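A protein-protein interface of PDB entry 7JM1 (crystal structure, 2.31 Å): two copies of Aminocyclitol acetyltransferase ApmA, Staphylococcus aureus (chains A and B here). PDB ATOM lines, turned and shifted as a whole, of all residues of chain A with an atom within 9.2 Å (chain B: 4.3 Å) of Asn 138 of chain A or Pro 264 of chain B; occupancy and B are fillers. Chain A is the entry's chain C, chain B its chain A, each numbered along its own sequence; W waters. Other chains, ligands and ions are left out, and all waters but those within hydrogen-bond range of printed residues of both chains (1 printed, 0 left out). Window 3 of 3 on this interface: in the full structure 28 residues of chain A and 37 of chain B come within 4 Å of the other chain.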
ATOM      1  N   ASN A 134      -1.573  11.021  19.947  1.00  0.00           N
ATOM      2  CA  ASN A 134      -2.140   9.958  19.132  1.00  0.00           C
ATOM      3  C   ASN A 134      -3.375  10.443  18.384  1.00  0.00           C
ATOM      4  O   ASN A 134      -4.134  11.284  18.872  1.00  0.00           O
ATOM      5  CB  ASN A 134      -2.535   8.765  20.001  1.00  0.00           C
ATOM      6  CG  ASN A 134      -1.346   8.071  20.618  1.00  0.00           C
ATOM      7  OD1 ASN A 134      -0.274   8.007  20.019  1.00  0.00           O
ATOM      8  ND2 ASN A 134      -1.529   7.545  21.825  1.00  0.00           N
ATOM      9  N   HIS A 135      -3.588   9.881  17.197  1.00  0.00           N
ATOM     10  CA  HIS A 135      -4.901   9.953  16.578  1.00  0.00           C
ATOM     11  C   HIS A 135      -5.893   9.102  17.375  1.00  0.00           C
ATOM     12  O   HIS A 135      -5.516   8.321  18.255  1.00  0.00           O
ATOM     13  CB  HIS A 135      -4.847   9.464  15.132  1.00  0.00           C
ATOM     14  CG  HIS A 135      -3.970  10.287  14.243  1.00  0.00           C
ATOM     15  ND1 HIS A 135      -3.962  10.145  12.871  1.00  0.00           N
ATOM     16  CD2 HIS A 135      -3.070  11.258  14.525  1.00  0.00           C
ATOM     17  CE1 HIS A 135      -3.096  10.994  12.348  1.00  0.00           C
ATOM     18  NE2 HIS A 135      -2.542  11.681  13.329  1.00  0.00           N
ATOM     19  N   GLN A 136      -7.178   9.253  17.053  1.00  0.00           N
ATOM     20  CA  GLN A 136      -8.190   8.370  17.623  1.00  0.00           C
ATOM     21  C   GLN A 136      -7.898   6.925  17.233  1.00  0.00           C
ATOM     22  O   GLN A 136      -7.488   6.637  16.107  1.00  0.00           O
ATOM     23  CB  GLN A 136      -9.590   8.778  17.151  1.00  0.00           C
ATOM     24  CG  GLN A 136      -9.889   8.451  15.698  1.00  0.00           C
ATOM     25  CD  GLN A 136      -9.279   9.458  14.743  1.00  0.00           C
ATOM     26  OE1 GLN A 136      -8.829  10.531  15.158  1.00  0.00           O
ATOM     27  NE2 GLN A 136      -9.250   9.115  13.458  1.00  0.00           N
ATOM     28  N   LEU A 137      -8.104   6.009  18.178  1.00  0.00           N
ATOM     29  CA  LEU A 137      -7.754   4.615  17.958  1.00  0.00           C
ATOM     30  C   LEU A 137      -8.931   3.658  18.032  1.00  0.00           C
ATOM     31  O   LEU A 137      -8.751   2.468  17.754  1.00  0.00           O
ATOM     32  CB  LEU A 137      -6.681   4.173  18.967  1.00  0.00           C
ATOM     33  CG  LEU A 137      -5.389   4.990  18.882  1.00  0.00           C
ATOM     34  CD1 LEU A 137      -4.509   4.799  20.116  1.00  0.00           C
ATOM     35  CD2 LEU A 137      -4.642   4.629  17.615  1.00  0.00           C
ATOM     36  N   ASN A 138     -10.121   4.126  18.386  1.00  0.00           N
ATOM     37  CA  ASN A 138     -11.272   3.248  18.544  1.00  0.00           C
ATOM     38  C   ASN A 138     -12.410   3.661  17.616  1.00  0.00           C
ATOM     39  O   ASN A 138     -13.588   3.500  17.933  1.00  0.00           O
ATOM     40  CB  ASN A 138     -11.715   3.208  20.005  1.00  0.00           C
ATOM     41  CG  ASN A 138     -10.641   2.611  20.917  1.00  0.00           C
ATOM     42  OD1 ASN A 138      -9.762   3.322  21.413  1.00  0.00           O
ATOM     43  ND2 ASN A 138     -10.702   1.297  21.125  1.00  0.00           N
ATOM     44  N   MET A 139     -12.050   4.188  16.458  1.00  0.00           N
ATOM     45  CA  MET A 139     -12.994   4.556  15.422  1.00  0.00           C
ATOM     46  C   MET A 139     -12.744   3.635  14.236  1.00  0.00           C
ATOM     47  O   MET A 139     -11.769   2.876  14.243  1.00  0.00           O
ATOM     48  CB  MET A 139     -12.797   6.026  15.064  1.00  0.00           C
ATOM     49  CG  MET A 139     -13.304   6.969  16.144  1.00  0.00           C
ATOM     50  SD  MET A 139     -13.782   8.713  15.433  1.00  0.00           S
ATOM     51  CE  MET A 139     -12.913   9.891  16.606  1.00  0.00           C
ATOM     52  N   THR A 140     -13.614   3.679  13.222  1.00  0.00           N
ATOM     53  CA  THR A 140     -13.393   2.838  12.049  1.00  0.00           C
ATOM     54  C   THR A 140     -12.158   3.293  11.272  1.00  0.00           C
ATOM     55  O   THR A 140     -11.472   2.471  10.653  1.00  0.00           O
ATOM     56  CB  THR A 140     -14.640   2.851  11.157  1.00  0.00           C
ATOM     57  OG1 THR A 140     -15.772   2.390  11.907  1.00  0.00           O
ATOM     58  CG2 THR A 140     -14.461   1.971   9.920  1.00  0.00           C
ATOM     59  N   PHE A 141     -11.843   4.582  11.322  1.00  0.00           N
ATOM     60  CA  PHE A 141     -10.695   5.151  10.636  1.00  0.00           C
ATOM     61  C   PHE A 141      -9.684   5.662  11.651  1.00  0.00           C
ATOM     62  O   PHE A 141     -10.022   5.971  12.799  1.00  0.00           O
ATOM     63  CB  PHE A 141     -11.124   6.292   9.703  1.00  0.00           C
ATOM     64  CG  PHE A 141     -11.795   7.441  10.410  1.00  0.00           C
ATOM     65  CD1 PHE A 141     -13.146   7.391  10.727  1.00  0.00           C
ATOM     66  CD2 PHE A 141     -11.073   8.581  10.749  1.00  0.00           C
ATOM     67  CE1 PHE A 141     -13.766   8.459  11.374  1.00  0.00           C
ATOM     68  CE2 PHE A 141     -11.686   9.650  11.394  1.00  0.00           C
ATOM     69  CZ  PHE A 141     -13.027   9.593  11.707  1.00  0.00           C
ATOM     70  N   VAL A 142      -8.426   5.735  11.217  1.00  0.00           N
ATOM     71  CA  VAL A 142      -7.357   6.319  12.023  1.00  0.00           C
ATOM     72  C   VAL A 142      -6.887   7.656  11.469  1.00  0.00           C
ATOM     73  O   VAL A 142      -6.220   8.417  12.193  1.00  0.00           O
ATOM     74  CB  VAL A 142      -6.169   5.341  12.170  1.00  0.00           C
ATOM     75  CG1 VAL A 142      -5.360   5.264  10.883  1.00  0.00           C
ATOM     76  CG2 VAL A 142      -5.293   5.710  13.370  1.00  0.00           C
ATOM     77  N   LYS A 161     -17.159  13.186  20.044  1.00  0.00           N
ATOM     78  CA  LYS A 161     -16.659  11.895  20.492  1.00  0.00           C
ATOM     79  C   LYS A 161     -15.155  11.905  20.735  1.00  0.00           C
ATOM     80  O   LYS A 161     -14.666  11.124  21.555  1.00  0.00           O
ATOM     81  CB  LYS A 161     -17.067  10.800  19.502  1.00  0.00           C
ATOM     82  CG  LYS A 161     -18.460  10.250  19.834  1.00  0.00           C
ATOM     83  CD  LYS A 161     -18.751   8.841  19.311  1.00  0.00           C
ATOM     84  CE  LYS A 161     -17.980   7.734  20.033  1.00  0.00           C
ATOM     85  NZ  LYS A 161     -16.515   7.730  19.733  1.00  0.00           N
ATOM     86  N   LEU A 162     -14.401  12.785  20.077  1.00  0.00           N
ATOM     87  CA  LEU A 162     -12.999  12.932  20.459  1.00  0.00           C
ATOM     88  C   LEU A 162     -12.871  13.428  21.898  1.00  0.00           C
ATOM     89  O   LEU A 162     -11.966  13.011  22.630  1.00  0.00           O
ATOM     90  CB  LEU A 162     -12.286  13.885  19.504  1.00  0.00           C
ATOM     91  CG  LEU A 162     -11.990  13.358  18.101  1.00  0.00           C
ATOM     92  CD1 LEU A 162     -11.306  14.437  17.287  1.00  0.00           C
ATOM     93  CD2 LEU A 162     -11.116  12.131  18.184  1.00  0.00           C
ATOM     94  N   LYS A 164     -14.897  12.922  24.450  1.00  0.00           N
ATOM     95  CA  LYS A 164     -15.259  11.906  25.428  1.00  0.00           C
ATOM     96  C   LYS A 164     -14.294  10.725  25.443  1.00  0.00           C
ATOM     97  O   LYS A 164     -14.306   9.948  26.403  1.00  0.00           O
ATOM     98  CB  LYS A 164     -16.693  11.411  25.177  1.00  0.00           C
ATOM     99  CG  LYS A 164     -16.899  10.686  23.849  1.00  0.00           C
ATOM    100  CD  LYS A 164     -16.545   9.197  23.917  1.00  0.00           C
ATOM    101  CE  LYS A 164     -16.031   8.732  22.575  1.00  0.00           C
ATOM    102  NZ  LYS A 164     -15.206   7.496  22.562  1.00  0.00           N
ATOM    103  N   ASP A 165     -13.483  10.563  24.406  1.00  0.00           N
ATOM    104  CA  ASP A 165     -12.543   9.448  24.313  1.00  0.00           C
ATOM    105  C   ASP A 165     -11.594   9.450  25.510  1.00  0.00           C
ATOM    106  O   ASP A 165     -10.824  10.408  25.680  1.00  0.00           O
ATOM    107  CB  ASP A 165     -11.761   9.544  23.006  1.00  0.00           C
ATOM    108  CG  ASP A 165     -10.969   8.281  22.686  1.00  0.00           C
ATOM    109  OD1 ASP A 165     -10.594   7.540  23.623  1.00  0.00           O
ATOM    110  OD2 ASP A 165     -10.706   8.040  21.483  1.00  0.00           O
ATOM    111  N   PRO A 166     -11.608   8.413  26.352  1.00  0.00           N
ATOM    112  CA  PRO A 166     -10.746   8.419  27.547  1.00  0.00           C
ATOM    113  C   PRO A 166      -9.262   8.253  27.246  1.00  0.00           C
ATOM    114  O   PRO A 166      -8.447   8.403  28.165  1.00  0.00           O
ATOM    115  CB  PRO A 166     -11.282   7.237  28.368  1.00  0.00           C
ATOM    116  CG  PRO A 166     -11.893   6.322  27.351  1.00  0.00           C
ATOM    117  CD  PRO A 166     -12.465   7.215  26.284  1.00  0.00           C
ATOM    118  N   LYS A 167      -8.882   7.962  26.003  1.00  0.00           N
ATOM    119  CA  LYS A 167      -7.481   7.810  25.632  1.00  0.00           C
ATOM    120  C   LYS A 167      -6.843   9.115  25.180  1.00  0.00           C
ATOM    121  O   LYS A 167      -5.657   9.119  24.837  1.00  0.00           O
ATOM    122  CB  LYS A 167      -7.340   6.755  24.528  1.00  0.00           C
ATOM    123  CG  LYS A 167      -7.422   5.325  25.046  1.00  0.00           C
ATOM    124  CD  LYS A 167      -8.118   4.399  24.062  1.00  0.00           C
ATOM    125  CE  LYS A 167      -7.181   3.285  23.596  1.00  0.00           C
ATOM    126  NZ  LYS A 167      -7.911   2.030  23.242  1.00  0.00           N
ATOM    127  N   HIS A 168      -7.601  10.210  25.160  1.00  0.00           N
ATOM    128  CA  HIS A 168      -7.117  11.557  24.872  1.00  0.00           C
ATOM    129  C   HIS A 168      -6.454  11.679  23.503  1.00  0.00           C
ATOM    130  O   HIS A 168      -5.293  12.104  23.419  1.00  0.00           O
ATOM    131  CB  HIS A 168      -6.131  12.005  25.955  1.00  0.00           C
ATOM    132  CG  HIS A 168      -6.596  11.724  27.348  1.00  0.00           C
ATOM    133  ND1 HIS A 168      -7.775  12.227  27.855  1.00  0.00           N
ATOM    134  CD2 HIS A 168      -6.043  10.987  28.341  1.00  0.00           C
ATOM    135  CE1 HIS A 168      -7.927  11.815  29.102  1.00  0.00           C
ATOM    136  NE2 HIS A 168      -6.890  11.061  29.420  1.00  0.00           N
ATOM    137  N   PRO A 169      -7.144  11.354  22.409  1.00  0.00           N
ATOM    138  CA  PRO A 169      -6.553  11.604  21.091  1.00  0.00           C
ATOM    139  C   PRO A 169      -6.388  13.101  20.872  1.00  0.00           C
ATOM    140  O   PRO A 169      -7.200  13.908  21.337  1.00  0.00           O
ATOM    141  CB  PRO A 169      -7.567  10.991  20.122  1.00  0.00           C
ATOM    142  CG  PRO A 169      -8.867  11.092  20.850  1.00  0.00           C
ATOM    143  CD  PRO A 169      -8.548  10.912  22.309  1.00  0.00           C
ATOM    144  N   PHE B 233      -9.146  -4.601  14.631  1.00  0.00           N
ATOM    145  CA  PHE B 233     -10.520  -5.077  14.575  1.00  0.00           C
ATOM    146  C   PHE B 233     -10.550  -6.599  14.576  1.00  0.00           C
ATOM    147  O   PHE B 233      -9.535  -7.269  14.359  1.00  0.00           O
ATOM    148  CB  PHE B 233     -11.240  -4.552  13.327  1.00  0.00           C
ATOM    149  CG  PHE B 233     -11.243  -3.049  13.199  1.00  0.00           C
ATOM    150  CD1 PHE B 233     -11.991  -2.265  14.060  1.00  0.00           C
ATOM    151  CD2 PHE B 233     -10.504  -2.424  12.209  1.00  0.00           C
ATOM    152  CE1 PHE B 233     -11.997  -0.880  13.940  1.00  0.00           C
ATOM    153  CE2 PHE B 233     -10.500  -1.038  12.089  1.00  0.00           C
ATOM    154  CZ  PHE B 233     -11.249  -0.269  12.951  1.00  0.00           C
ATOM    155  N   MET B 237     -14.672  -8.161  10.983  1.00  0.00           N
ATOM    156  CA  MET B 237     -14.681  -6.735  10.689  1.00  0.00           C
ATOM    157  C   MET B 237     -13.666  -6.408   9.600  1.00  0.00           C
ATOM    158  O   MET B 237     -13.945  -5.627   8.690  1.00  0.00           O
ATOM    159  CB  MET B 237     -14.380  -5.922  11.947  1.00  0.00           C
ATOM    160  CG  MET B 237     -14.167  -4.435  11.679  1.00  0.00           C
ATOM    161  SD  MET B 237     -15.826  -3.478  11.344  1.00  0.00           S
ATOM    162  CE  MET B 237     -15.252  -1.683  11.838  1.00  0.00           C
ATOM    163  N   ILE B 262     -17.488   6.623  12.662  1.00  0.00           N
ATOM    164  CA  ILE B 262     -17.061   6.940  14.017  1.00  0.00           C
ATOM    165  C   ILE B 262     -17.124   5.704  14.915  1.00  0.00           C
ATOM    166  O   ILE B 262     -16.218   5.465  15.724  1.00  0.00           O
ATOM    167  CB  ILE B 262     -17.913   8.101  14.554  1.00  0.00           C
ATOM    168  CG1 ILE B 262     -17.361   9.431  14.036  1.00  0.00           C
ATOM    169  CG2 ILE B 262     -17.956   8.085  16.061  1.00  0.00           C
ATOM    170  CD1 ILE B 262     -18.197  10.637  14.442  1.00  0.00           C
ATOM    171  N   SER B 263     -18.172   4.890  14.782  1.00  0.00           N
ATOM    172  CA  SER B 263     -18.369   3.750  15.669  1.00  0.00           C
ATOM    173  C   SER B 263     -18.210   2.451  14.895  1.00  0.00           C
ATOM    174  O   SER B 263     -19.024   2.168  14.001  1.00  0.00           O
ATOM    175  CB  SER B 263     -19.745   3.812  16.330  1.00  0.00           C
ATOM    176  OG  SER B 263     -20.136   2.536  16.812  1.00  0.00           O
ATOM    177  N   PRO B 264     -17.190   1.642  15.192  1.00  0.00           N
ATOM    178  CA  PRO B 264     -17.029   0.374  14.458  1.00  0.00           C
ATOM    179  C   PRO B 264     -18.195  -0.577  14.638  1.00  0.00           C
ATOM    180  O   PRO B 264     -18.497  -1.351  13.721  1.00  0.00           O
ATOM    181  CB  PRO B 264     -15.728  -0.202  15.038  1.00  0.00           C
ATOM    182  CG  PRO B 264     -14.978   1.003  15.552  1.00  0.00           C
ATOM    183  CD  PRO B 264     -16.052   1.913  16.089  1.00  0.00           C
ATOM    184  N   GLU B 265     -18.872  -0.537  15.788  1.00  0.00           N
ATOM    185  CA  GLU B 265     -20.024  -1.406  15.995  1.00  0.00           C
ATOM    186  C   GLU B 265     -21.173  -1.026  15.071  1.00  0.00           C
ATOM    187  O   GLU B 265     -21.840  -1.902  14.512  1.00  0.00           O
ATOM    188  CB  GLU B 265     -20.472  -1.356  17.455  1.00  0.00           C
ATOM    189  CG  GLU B 265     -21.540  -2.392  17.802  1.00  0.00           C
ATOM    190  CD  GLU B 265     -21.905  -2.401  19.281  1.00  0.00           C
ATOM    191  OE1 GLU B 265     -23.092  -2.627  19.603  1.00  0.00           O
ATOM    192  OE2 GLU B 265     -21.004  -2.187  20.121  1.00  0.00           O
ATOM    193  N   LEU B 266     -21.421   0.274  14.899  1.00  0.00           N
ATOM    194  CA  LEU B 266     -22.432   0.697  13.936  1.00  0.00           C
ATOM    195  C   LEU B 266     -22.018   0.354  12.509  1.00  0.00           C
ATOM    196  O   LEU B 266     -22.880   0.099  11.660  1.00  0.00           O
ATOM    197  CB  LEU B 266     -22.694   2.195  14.071  1.00  0.00           C
ATOM    198  CG  LEU B 266     -23.369   2.617  15.379  1.00  0.00           C
ATOM    199  CD1 LEU B 266     -23.507   4.131  15.458  1.00  0.00           C
ATOM    200  CD2 LEU B 266     -24.730   1.943  15.541  1.00  0.00           C
ATOM    201  N   PHE B 267     -20.713   0.329  12.234  1.00  0.00           N
ATOM    202  CA  PHE B 267     -20.245  -0.030  10.901  1.00  0.00           C
ATOM    203  C   PHE B 267     -20.630  -1.465  10.555  1.00  0.00           C
ATOM    204  O   PHE B 267     -21.107  -1.737   9.448  1.00  0.00           O
ATOM    205  CB  PHE B 267     -18.730   0.165  10.803  1.00  0.00           C
ATOM    206  CG  PHE B 267     -18.195   0.033   9.405  1.00  0.00           C
ATOM    207  CD1 PHE B 267     -17.873  -1.211   8.883  1.00  0.00           C
ATOM    208  CD2 PHE B 267     -18.024   1.153   8.608  1.00  0.00           C
ATOM    209  CE1 PHE B 267     -17.391  -1.336   7.591  1.00  0.00           C
ATOM    210  CE2 PHE B 267     -17.539   1.041   7.321  1.00  0.00           C
ATOM    211  CZ  PHE B 267     -17.222  -0.210   6.809  1.00  0.00           C
ATOM    212  N   MET B 268     -20.436  -2.394  11.494  1.00  0.00           N
ATOM    213  CA  MET B 268     -20.735  -3.812  11.261  1.00  0.00           C
ATOM    214  C   MET B 268     -22.224  -4.082  11.152  1.00  0.00           C
ATOM    215  O   MET B 268     -22.645  -4.850  10.299  1.00  0.00           O
ATOM    216  CB  MET B 268     -20.154  -4.690  12.371  1.00  0.00           C
ATOM    217  CG  MET B 268     -18.699  -5.053  12.188  1.00  0.00           C
ATOM    218  SD  MET B 268     -18.255  -5.703  10.410  1.00  0.00           S
ATOM    219  CE  MET B 268     -19.170  -7.388  10.418  1.00  0.00           C
HETATM  220  O   HOH W   1     -16.227   4.935  18.409  1.00  0.00           O
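Leu 137 of chain A touches none of the printed residues of chain B.
Asn 138 of chain A touches just these residues of chain B: Ile 262 (3.96 Å) and Pro 264 (3.5 Å).
Of the printed residues of chain B, Met 139 of chain A touches Phe 233 (3.4 Å), Ile 262 (3.3 Å) and Pro 264 (3.7 Å).
Printed residues of chain B within 4 Å of Thr 140 of chain A: Phe 233, Ser 263, Pro 264 and Phe 267.
Printed residues of chain B within 4 Å of Lys 161 of chain A: Ile 262 (3.4 Å).
Asp 165 of chain A touches none of the printed residues of chain B.
Of the printed residues of chain A, Phe 233 of chain B touches Met 139 and Thr 140.
Of chain A, only Asn 138, Met 139 and Thr 140 come within 4 Å of Pro 264 of chain B.
The nearest printed residue of chain A that does not touch Phe 233 of chain B is Phe 141 of chain A (5.2 Å).
OG of Ser 263 of chain B lies close to N of Glu 265 of chain B (3.5 Å).
The side-chain amino group of Lys 167 of chain A is in hydrogen-bond range of the side-chain amide oxygen of Asn 138 of chain A, 2.9 Å away.
The backbone NH (N) of Leu 266 of chain B lies within hydrogen-bond range of the side-chain hydroxyl (OG) of Ser 263 of chain B (3.2 Å).
No position is printed for both chains.
Water W1 lies within hydrogen-bond range of the backbone carbonyl oxygen (O) of Ile 262 of chain B (2.7 Å), the backbone carbonyl oxygen (O) of Asn 138 of chain A (3.0 Å) and the side-chain amino group (NZ) of Lys 161 of chain A (3.1 Å).
Printed residues of chain A that touch a printed residue of chain B: Asn 138, Met 139, Thr 140 and Lys 161.
Of the 9 printed residues of chain B, 5 touch a printed residue of chain A.
Hydrophobic or aromatic side chains of chain B that line the printed part of chain A: Phe 233, Ile 262, Pro 264 and Phe 267.
Among the printed residues, no Asp or Glu carboxylate lies within 4 Å of a Lys or Arg side-chain nitrogen of the other chain.
Among the printed residues, pairs that only touch across the chains: Met 139 of chain A with Ile 262 of chain B, Lys 161 of chain A with Ile 262 of chain B, Met 139 of chain A with Phe 233 of chain B, Asn 138 of chain A with Pro 264 of chain B, Thr 140 of chain A with Pro 264 of chain B, Thr 140 of chain A with Phe 233 of chain B, Met 139 of chain A with Pro 264 of chain B, Thr 140 of chain A with Ser 263 of chain B, Thr 140 of chain A with Phe 267 of chain B and Asn 138 of chain A with Ile 262 of chain B.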
